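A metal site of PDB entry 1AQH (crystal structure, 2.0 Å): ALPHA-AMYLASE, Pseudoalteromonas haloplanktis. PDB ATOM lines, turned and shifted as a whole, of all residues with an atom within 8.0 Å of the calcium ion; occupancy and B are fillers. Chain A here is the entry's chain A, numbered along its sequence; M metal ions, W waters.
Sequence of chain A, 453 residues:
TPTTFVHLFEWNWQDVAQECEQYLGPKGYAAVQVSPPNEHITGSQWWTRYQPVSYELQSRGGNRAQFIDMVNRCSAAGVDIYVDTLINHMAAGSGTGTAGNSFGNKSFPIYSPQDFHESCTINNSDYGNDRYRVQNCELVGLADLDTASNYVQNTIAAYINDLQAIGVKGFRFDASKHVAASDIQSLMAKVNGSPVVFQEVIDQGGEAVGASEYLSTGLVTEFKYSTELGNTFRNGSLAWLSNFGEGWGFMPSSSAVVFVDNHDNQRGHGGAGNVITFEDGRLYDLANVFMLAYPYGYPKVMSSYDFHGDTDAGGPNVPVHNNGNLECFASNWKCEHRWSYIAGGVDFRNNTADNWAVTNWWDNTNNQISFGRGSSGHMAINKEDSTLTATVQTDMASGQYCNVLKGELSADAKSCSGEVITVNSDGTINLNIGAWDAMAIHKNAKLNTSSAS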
ATOM      1  N   ILE A  87     -19.475   2.481  10.309  1.00  0.00           N
ATOM      2  CA  ILE A  87     -18.525   1.400  10.036  1.00  0.00           C
ATOM      3  C   ILE A  87     -17.101   1.872   9.700  1.00  0.00           C
ATOM      4  O   ILE A  87     -16.168   1.069   9.709  1.00  0.00           O
ATOM      5  CB  ILE A  87     -19.021   0.501   8.881  1.00  0.00           C
ATOM      6  CG1 ILE A  87     -19.100   1.306   7.579  1.00  0.00           C
ATOM      7  CG2 ILE A  87     -20.369  -0.110   9.234  1.00  0.00           C
ATOM      8  CD1 ILE A  87     -19.198   0.463   6.345  1.00  0.00           C
ATOM      9  N   ASN A  88     -16.933   3.158   9.464  1.00  0.00           N
ATOM     10  CA  ASN A  88     -15.638   3.718   9.067  1.00  0.00           C
ATOM     11  C   ASN A  88     -14.717   4.283  10.144  1.00  0.00           C
ATOM     12  O   ASN A  88     -13.497   4.115  10.072  1.00  0.00           O
ATOM     13  CB  ASN A  88     -15.891   4.805   7.992  1.00  0.00           C
ATOM     14  CG  ASN A  88     -14.604   5.428   7.447  1.00  0.00           C
ATOM     15  OD1 ASN A  88     -13.840   4.769   6.736  1.00  0.00           O
ATOM     16  ND2 ASN A  88     -14.379   6.697   7.766  1.00  0.00           N
ATOM     17  N   HIS A  89     -15.282   4.906  11.172  1.00  0.00           N
ATOM     18  CA  HIS A  89     -14.444   5.583  12.149  1.00  0.00           C
ATOM     19  C   HIS A  89     -14.963   5.673  13.577  1.00  0.00           C
ATOM     20  O   HIS A  89     -16.092   5.272  13.881  1.00  0.00           O
ATOM     21  CB  HIS A  89     -14.264   7.017  11.639  1.00  0.00           C
ATOM     22  CG  HIS A  89     -15.576   7.697  11.333  1.00  0.00           C
ATOM     23  ND1 HIS A  89     -16.130   7.703  10.071  1.00  0.00           N
ATOM     24  CD2 HIS A  89     -16.485   8.282  12.153  1.00  0.00           C
ATOM     25  CE1 HIS A  89     -17.339   8.260  10.124  1.00  0.00           C
ATOM     26  NE2 HIS A  89     -17.570   8.617  11.371  1.00  0.00           N
ATOM     27  N   HIS A 117      -5.937   2.648  11.113  1.00  0.00           N
ATOM     28  CA  HIS A 117      -4.921   2.861  10.095  1.00  0.00           C
ATOM     29  C   HIS A 117      -4.048   4.001  10.626  1.00  0.00           C
ATOM     30  O   HIS A 117      -4.523   4.819  11.444  1.00  0.00           O
ATOM     31  CB  HIS A 117      -5.547   3.325   8.790  1.00  0.00           C
ATOM     32  CG  HIS A 117      -6.384   2.284   8.096  1.00  0.00           C
ATOM     33  ND1 HIS A 117      -7.587   2.574   7.514  1.00  0.00           N
ATOM     34  CD2 HIS A 117      -6.156   0.968   7.864  1.00  0.00           C
ATOM     35  CE1 HIS A 117      -8.072   1.496   6.941  1.00  0.00           C
ATOM     36  NE2 HIS A 117      -7.229   0.501   7.143  1.00  0.00           N
ATOM     37  N   ILE A 122      -7.346  13.080   4.470  1.00  0.00           N
ATOM     38  CA  ILE A 122      -7.952  12.938   3.148  1.00  0.00           C
ATOM     39  C   ILE A 122      -8.086  14.348   2.582  1.00  0.00           C
ATOM     40  O   ILE A 122      -8.748  15.197   3.188  1.00  0.00           O
ATOM     41  CB  ILE A 122      -9.373  12.336   3.208  1.00  0.00           C
ATOM     42  CG1 ILE A 122      -9.330  10.865   3.614  1.00  0.00           C
ATOM     43  CG2 ILE A 122     -10.059  12.480   1.853  1.00  0.00           C
ATOM     44  CD1 ILE A 122     -10.688  10.202   3.599  1.00  0.00           C
ATOM     45  N   TYR A 132      -6.665   4.872  -2.387  1.00  0.00           N
ATOM     46  CA  TYR A 132      -5.965   4.425  -1.201  1.00  0.00           C
ATOM     47  C   TYR A 132      -6.103   5.448  -0.081  1.00  0.00           C
ATOM     48  O   TYR A 132      -6.398   5.087   1.047  1.00  0.00           O
ATOM     49  CB  TYR A 132      -4.483   4.134  -1.505  1.00  0.00           C
ATOM     50  CG  TYR A 132      -3.679   3.802  -0.278  1.00  0.00           C
ATOM     51  CD1 TYR A 132      -3.593   2.497   0.202  1.00  0.00           C
ATOM     52  CD2 TYR A 132      -3.066   4.820   0.461  1.00  0.00           C
ATOM     53  CE1 TYR A 132      -2.928   2.201   1.399  1.00  0.00           C
ATOM     54  CE2 TYR A 132      -2.394   4.545   1.657  1.00  0.00           C
ATOM     55  CZ  TYR A 132      -2.335   3.234   2.122  1.00  0.00           C
ATOM     56  OH  TYR A 132      -1.698   2.981   3.312  1.00  0.00           O
ATOM     57  N   ARG A 133      -5.878   6.727  -0.396  1.00  0.00           N
ATOM     58  CA  ARG A 133      -6.014   7.789   0.618  1.00  0.00           C
ATOM     59  C   ARG A 133      -7.467   7.971   1.071  1.00  0.00           C
ATOM     60  O   ARG A 133      -7.735   8.231   2.252  1.00  0.00           O
ATOM     61  CB  ARG A 133      -5.459   9.121   0.118  1.00  0.00           C
ATOM     62  CG  ARG A 133      -3.946   9.146  -0.052  1.00  0.00           C
ATOM     63  CD  ARG A 133      -3.448  10.576   0.002  1.00  0.00           C
ATOM     64  NE  ARG A 133      -2.525  10.750   1.116  1.00  0.00           N
ATOM     65  CZ  ARG A 133      -2.563  11.747   1.981  1.00  0.00           C
ATOM     66  NH1 ARG A 133      -3.480  12.695   1.881  1.00  0.00           N
ATOM     67  NH2 ARG A 133      -1.678  11.815   2.962  1.00  0.00           N
ATOM     68  N   VAL A 134      -8.404   7.852   0.118  1.00  0.00           N
ATOM     69  CA  VAL A 134      -9.829   7.980   0.412  1.00  0.00           C
ATOM     70  C   VAL A 134     -10.287   6.899   1.429  1.00  0.00           C
ATOM     71  O   VAL A 134     -11.051   7.185   2.357  1.00  0.00           O
ATOM     72  CB  VAL A 134     -10.677   7.842  -0.902  1.00  0.00           C
ATOM     73  CG1 VAL A 134     -12.176   7.633  -0.580  1.00  0.00           C
ATOM     74  CG2 VAL A 134     -10.509   9.088  -1.763  1.00  0.00           C
ATOM     75  N   GLN A 135      -9.781   5.681   1.268  1.00  0.00           N
ATOM     76  CA  GLN A 135     -10.183   4.585   2.140  1.00  0.00           C
ATOM     77  C   GLN A 135      -9.276   4.285   3.329  1.00  0.00           C
ATOM     78  O   GLN A 135      -9.680   3.547   4.235  1.00  0.00           O
ATOM     79  CB  GLN A 135     -10.454   3.336   1.297  1.00  0.00           C
ATOM     80  CG  GLN A 135     -11.506   3.585   0.221  1.00  0.00           C
ATOM     81  CD  GLN A 135     -11.814   2.379  -0.676  1.00  0.00           C
ATOM     82  OE1 GLN A 135     -11.005   1.443  -0.796  1.00  0.00           O
ATOM     83  NE2 GLN A 135     -12.986   2.403  -1.302  1.00  0.00           N
ATOM     84  N   ASN A 136      -8.084   4.865   3.362  1.00  0.00           N
ATOM     85  CA  ASN A 136      -7.177   4.574   4.476  1.00  0.00           C
ATOM     86  C   ASN A 136      -6.830   5.759   5.332  1.00  0.00           C
ATOM     87  O   ASN A 136      -6.327   5.593   6.438  1.00  0.00           O
ATOM     88  CB  ASN A 136      -5.893   3.891   3.979  1.00  0.00           C
ATOM     89  CG  ASN A 136      -6.149   2.489   3.446  1.00  0.00           C
ATOM     90  OD1 ASN A 136      -6.129   1.517   4.202  1.00  0.00           O
ATOM     91  ND2 ASN A 136      -6.417   2.379   2.155  1.00  0.00           N
ATOM     92  N   CYS A 137      -7.092   6.962   4.830  1.00  0.00           N
ATOM     93  CA  CYS A 137      -6.802   8.166   5.602  1.00  0.00           C
ATOM     94  C   CYS A 137      -8.038   8.640   6.344  1.00  0.00           C
ATOM     95  O   CYS A 137      -9.136   8.120   6.142  1.00  0.00           O
ATOM     96  CB  CYS A 137      -6.220   9.270   4.718  1.00  0.00           C
ATOM     97  SG  CYS A 137      -4.559   8.872   4.064  1.00  0.00           S
ATOM     98  N   GLU A 138      -7.853   9.657   7.180  1.00  0.00           N
ATOM     99  CA  GLU A 138      -8.911  10.228   8.001  1.00  0.00           C
ATOM    100  C   GLU A 138      -9.850  11.253   7.360  1.00  0.00           C
ATOM    101  O   GLU A 138      -9.413  12.208   6.731  1.00  0.00           O
ATOM    102  CB  GLU A 138      -8.312  10.819   9.265  1.00  0.00           C
ATOM    103  CG  GLU A 138      -7.526   9.820  10.109  1.00  0.00           C
ATOM    104  CD  GLU A 138      -6.737  10.482  11.238  1.00  0.00           C
ATOM    105  OE1 GLU A 138      -6.484  11.708  11.163  1.00  0.00           O
ATOM    106  OE2 GLU A 138      -6.358   9.774  12.190  1.00  0.00           O
ATOM    107  N   LEU A 139     -11.135  11.033   7.587  1.00  0.00           N
ATOM    108  CA  LEU A 139     -12.211  11.905   7.124  1.00  0.00           C
ATOM    109  C   LEU A 139     -12.356  12.976   8.228  1.00  0.00           C
ATOM    110  O   LEU A 139     -12.805  12.682   9.342  1.00  0.00           O
ATOM    111  CB  LEU A 139     -13.496  11.100   7.002  1.00  0.00           C
ATOM    112  CG  LEU A 139     -14.774  11.840   6.639  1.00  0.00           C
ATOM    113  CD1 LEU A 139     -14.645  12.434   5.236  1.00  0.00           C
ATOM    114  CD2 LEU A 139     -15.935  10.869   6.717  1.00  0.00           C
ATOM    115  N   LEU A 142     -11.316  12.129  11.858  1.00  0.00           N
ATOM    116  CA  LEU A 142     -11.963  11.018  12.535  1.00  0.00           C
ATOM    117  C   LEU A 142     -11.039   9.799  12.459  1.00  0.00           C
ATOM    118  O   LEU A 142     -10.532   9.477  11.383  1.00  0.00           O
ATOM    119  CB  LEU A 142     -13.310  10.697  11.862  1.00  0.00           C
ATOM    120  CG  LEU A 142     -14.552  11.530  12.213  1.00  0.00           C
ATOM    121  CD1 LEU A 142     -14.155  12.865  12.759  1.00  0.00           C
ATOM    122  CD2 LEU A 142     -15.466  11.679  11.009  1.00  0.00           C
ATOM    123  N   ALA A 143     -10.797   9.158  13.610  1.00  0.00           N
ATOM    124  CA  ALA A 143      -9.913   7.981  13.667  1.00  0.00           C
ATOM    125  C   ALA A 143     -10.404   6.917  12.678  1.00  0.00           C
ATOM    126  O   ALA A 143     -11.538   6.437  12.791  1.00  0.00           O
ATOM    127  CB  ALA A 143      -9.867   7.430  15.105  1.00  0.00           C
ATOM    128  N   ASP A 144      -9.571   6.579  11.694  1.00  0.00           N
ATOM    129  CA  ASP A 144      -9.966   5.617  10.672  1.00  0.00           C
ATOM    130  C   ASP A 144      -9.715   4.151  11.039  1.00  0.00           C
ATOM    131  O   ASP A 144      -8.571   3.700  11.088  1.00  0.00           O
ATOM    132  CB  ASP A 144      -9.271   5.957   9.353  1.00  0.00           C
ATOM    133  CG  ASP A 144     -10.016   5.430   8.140  1.00  0.00           C
ATOM    134  OD1 ASP A 144     -11.139   5.890   7.854  1.00  0.00           O
ATOM    135  OD2 ASP A 144      -9.468   4.558   7.449  1.00  0.00           O
ATOM    136  N   LEU A 145     -10.791   3.400  11.287  1.00  0.00           N
ATOM    137  CA  LEU A 145     -10.703   1.992  11.667  1.00  0.00           C
ATOM    138  C   LEU A 145     -10.066   1.091  10.620  1.00  0.00           C
ATOM    139  O   LEU A 145     -10.262   1.270   9.409  1.00  0.00           O
ATOM    140  CB  LEU A 145     -12.096   1.435  11.967  1.00  0.00           C
ATOM    141  CG  LEU A 145     -12.818   1.665  13.295  1.00  0.00           C
ATOM    142  CD1 LEU A 145     -14.258   1.180  13.180  1.00  0.00           C
ATOM    143  CD2 LEU A 145     -12.119   0.944  14.415  1.00  0.00           C
ATOM    144  N   ASP A 146      -9.310   0.103  11.087  1.00  0.00           N
ATOM    145  CA  ASP A 146      -8.706  -0.840  10.159  1.00  0.00           C
ATOM    146  C   ASP A 146      -9.808  -1.875   9.896  1.00  0.00           C
ATOM    147  O   ASP A 146      -9.926  -2.898  10.601  1.00  0.00           O
ATOM    148  CB  ASP A 146      -7.456  -1.477  10.761  1.00  0.00           C
ATOM    149  CG  ASP A 146      -6.764  -2.447   9.807  1.00  0.00           C
ATOM    150  OD1 ASP A 146      -7.222  -2.629   8.651  1.00  0.00           O
ATOM    151  OD2 ASP A 146      -5.753  -3.030  10.221  1.00  0.00           O
ATOM    152  N   THR A 147     -10.632  -1.606   8.885  1.00  0.00           N
ATOM    153  CA  THR A 147     -11.741  -2.470   8.540  1.00  0.00           C
ATOM    154  C   THR A 147     -11.354  -3.806   7.882  1.00  0.00           C
ATOM    155  O   THR A 147     -12.207  -4.611   7.547  1.00  0.00           O
ATOM    156  CB  THR A 147     -12.785  -1.692   7.716  1.00  0.00           C
ATOM    157  OG1 THR A 147     -12.147  -1.101   6.571  1.00  0.00           O
ATOM    158  CG2 THR A 147     -13.383  -0.572   8.575  1.00  0.00           C
ATOM    159  N   ALA A 175     -20.715   6.522   5.666  1.00  0.00           N
ATOM    160  CA  ALA A 175     -19.389   6.714   5.055  1.00  0.00           C
ATOM    161  C   ALA A 175     -18.821   5.455   4.368  1.00  0.00           C
ATOM    162  O   ALA A 175     -17.620   5.170   4.492  1.00  0.00           O
ATOM    163  CB  ALA A 175     -18.409   7.243   6.107  1.00  0.00           C
ATOM    164  N   SER A 176     -19.660   4.740   3.638  1.00  0.00           N
ATOM    165  CA  SER A 176     -19.236   3.527   2.964  1.00  0.00           C
ATOM    166  C   SER A 176     -18.140   3.725   1.921  1.00  0.00           C
ATOM    167  O   SER A 176     -17.317   2.840   1.724  1.00  0.00           O
ATOM    168  CB  SER A 176     -20.427   2.811   2.360  1.00  0.00           C
ATOM    169  OG  SER A 176     -21.230   2.238   3.364  1.00  0.00           O
ATOM    170  N   LYS A 177     -18.125   4.881   1.254  1.00  0.00           N
ATOM    171  CA  LYS A 177     -17.097   5.157   0.254  1.00  0.00           C
ATOM    172  C   LYS A 177     -15.688   5.095   0.847  1.00  0.00           C
ATOM    173  O   LYS A 177     -14.726   4.782   0.162  1.00  0.00           O
ATOM    174  CB  LYS A 177     -17.318   6.532  -0.374  1.00  0.00           C
ATOM    175  CG  LYS A 177     -16.251   6.902  -1.407  1.00  0.00           C
ATOM    176  CD  LYS A 177     -16.741   7.960  -2.378  1.00  0.00           C
ATOM    177  CE  LYS A 177     -16.647   9.357  -1.779  1.00  0.00           C
ATOM    178  NZ  LYS A 177     -17.224  10.337  -2.737  1.00  0.00           N
ATOM    179  N   HIS A 178     -15.584   5.363   2.151  1.00  0.00           N
ATOM    180  CA  HIS A 178     -14.302   5.365   2.821  1.00  0.00           C
ATOM    181  C   HIS A 178     -13.871   4.004   3.334  1.00  0.00           C
ATOM    182  O   HIS A 178     -12.910   3.896   4.091  1.00  0.00           O
ATOM    183  CB  HIS A 178     -14.309   6.438   3.896  1.00  0.00           C
ATOM    184  CG  HIS A 178     -14.619   7.804   3.383  1.00  0.00           C
ATOM    185  ND1 HIS A 178     -13.655   8.682   2.970  1.00  0.00           N
ATOM    186  CD2 HIS A 178     -15.811   8.421   3.165  1.00  0.00           C
ATOM    187  CE1 HIS A 178     -14.214   9.793   2.525  1.00  0.00           C
ATOM    188  NE2 HIS A 178     -15.530   9.661   2.630  1.00  0.00           N
ATOM    189  N   VAL A 179     -14.599   2.969   2.923  1.00  0.00           N
ATOM    190  CA  VAL A 179     -14.277   1.600   3.313  1.00  0.00           C
ATOM    191  C   VAL A 179     -14.281   0.759   2.047  1.00  0.00           C
ATOM    192  O   VAL A 179     -15.216   0.831   1.240  1.00  0.00           O
ATOM    193  CB  VAL A 179     -15.327   1.007   4.297  1.00  0.00           C
ATOM    194  CG1 VAL A 179     -15.001  -0.459   4.623  1.00  0.00           C
ATOM    195  CG2 VAL A 179     -15.373   1.836   5.555  1.00  0.00           C
ATOM    196  N   ALA A 180     -13.222  -0.018   1.843  1.00  0.00           N
ATOM    197  CA  ALA A 180     -13.135  -0.875   0.672  1.00  0.00           C
ATOM    198  C   ALA A 180     -14.338  -1.810   0.587  1.00  0.00           C
ATOM    199  O   ALA A 180     -14.744  -2.412   1.593  1.00  0.00           O
ATOM    200  CB  ALA A 180     -11.833  -1.683   0.684  1.00  0.00           C
ATOM    201  N   ASP A 183     -13.851  -5.014   2.196  1.00  0.00           N
ATOM    202  CA  ASP A 183     -13.890  -5.040   3.659  1.00  0.00           C
ATOM    203  C   ASP A 183     -15.350  -5.232   4.093  1.00  0.00           C
ATOM    204  O   ASP A 183     -15.626  -5.919   5.072  1.00  0.00           O
ATOM    205  CB  ASP A 183     -13.365  -3.745   4.274  1.00  0.00           C
ATOM    206  CG  ASP A 183     -11.863  -3.643   4.240  1.00  0.00           C
ATOM    207  OD1 ASP A 183     -11.201  -4.651   3.930  1.00  0.00           O
ATOM    208  OD2 ASP A 183     -11.359  -2.544   4.531  1.00  0.00           O
HETATM  209 CA    CA M   1     -11.575   4.103   6.066  1.00  0.00          CA
HETATM  210  O   HOH W   1     -12.042   2.729   8.032  1.00  0.00           O
HETATM  211  O   HOH W   2     -11.338   1.628   5.679  1.00  0.00           O
HETATM  212  O   HOH W   3     -10.895   6.413   4.931  1.00  0.00           O
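ND1 of His 178 is in hydrogen-bond range of O of Val 134 (3.1 Å).
The backbone carbonyl oxygen (O) of Asn 88 is in hydrogen-bond range of the backbone NH (N) of Leu 145.
A ring nitrogen (ND1) of His 89 is in hydrogen-bond range of the side-chain amide nitrogen (ND2) of Asn 88 (3.1 Å).
O of Asp 144 lies within hydrogen-bond range of N of His 117 (2.8 Å).
The backbone carbonyl oxygen (O) of Lys 177 is in hydrogen-bond range of the side-chain amide nitrogen (NE2) of Gln 135 (3.3 Å).
Within 4 Å of the calcium ion: Asn 88, Gln 135, Asp 144 and His 178.
The nearest printed residue that does not touch the calcium ion is Val 179 (4.5 Å).
The calcium ion is bound by the backbone carbonyl oxygen (O) of His 178, 2.4 Å away.
The calcium ion is bound by water W1.
OD1 of Asn 88 is bound to the calcium ion, at 2.5 Å.
Water W2 binds the calcium ion, 2.5 Å away.
The calcium ion is bound by the side-chain carboxylate (OD2) of Asp 144 (2.6 Å).
OD1 of Asp 144 is bound to the calcium ion.
Water W3 is bound to the calcium ion (2.7 Å).
The calcium ion is bound by O of Gln 135 (2.7 Å).
The calcium ion has eight donor atoms within binding distance.
Water W1 lies within hydrogen-bond range of O of Leu 145 and O of Asn 88.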
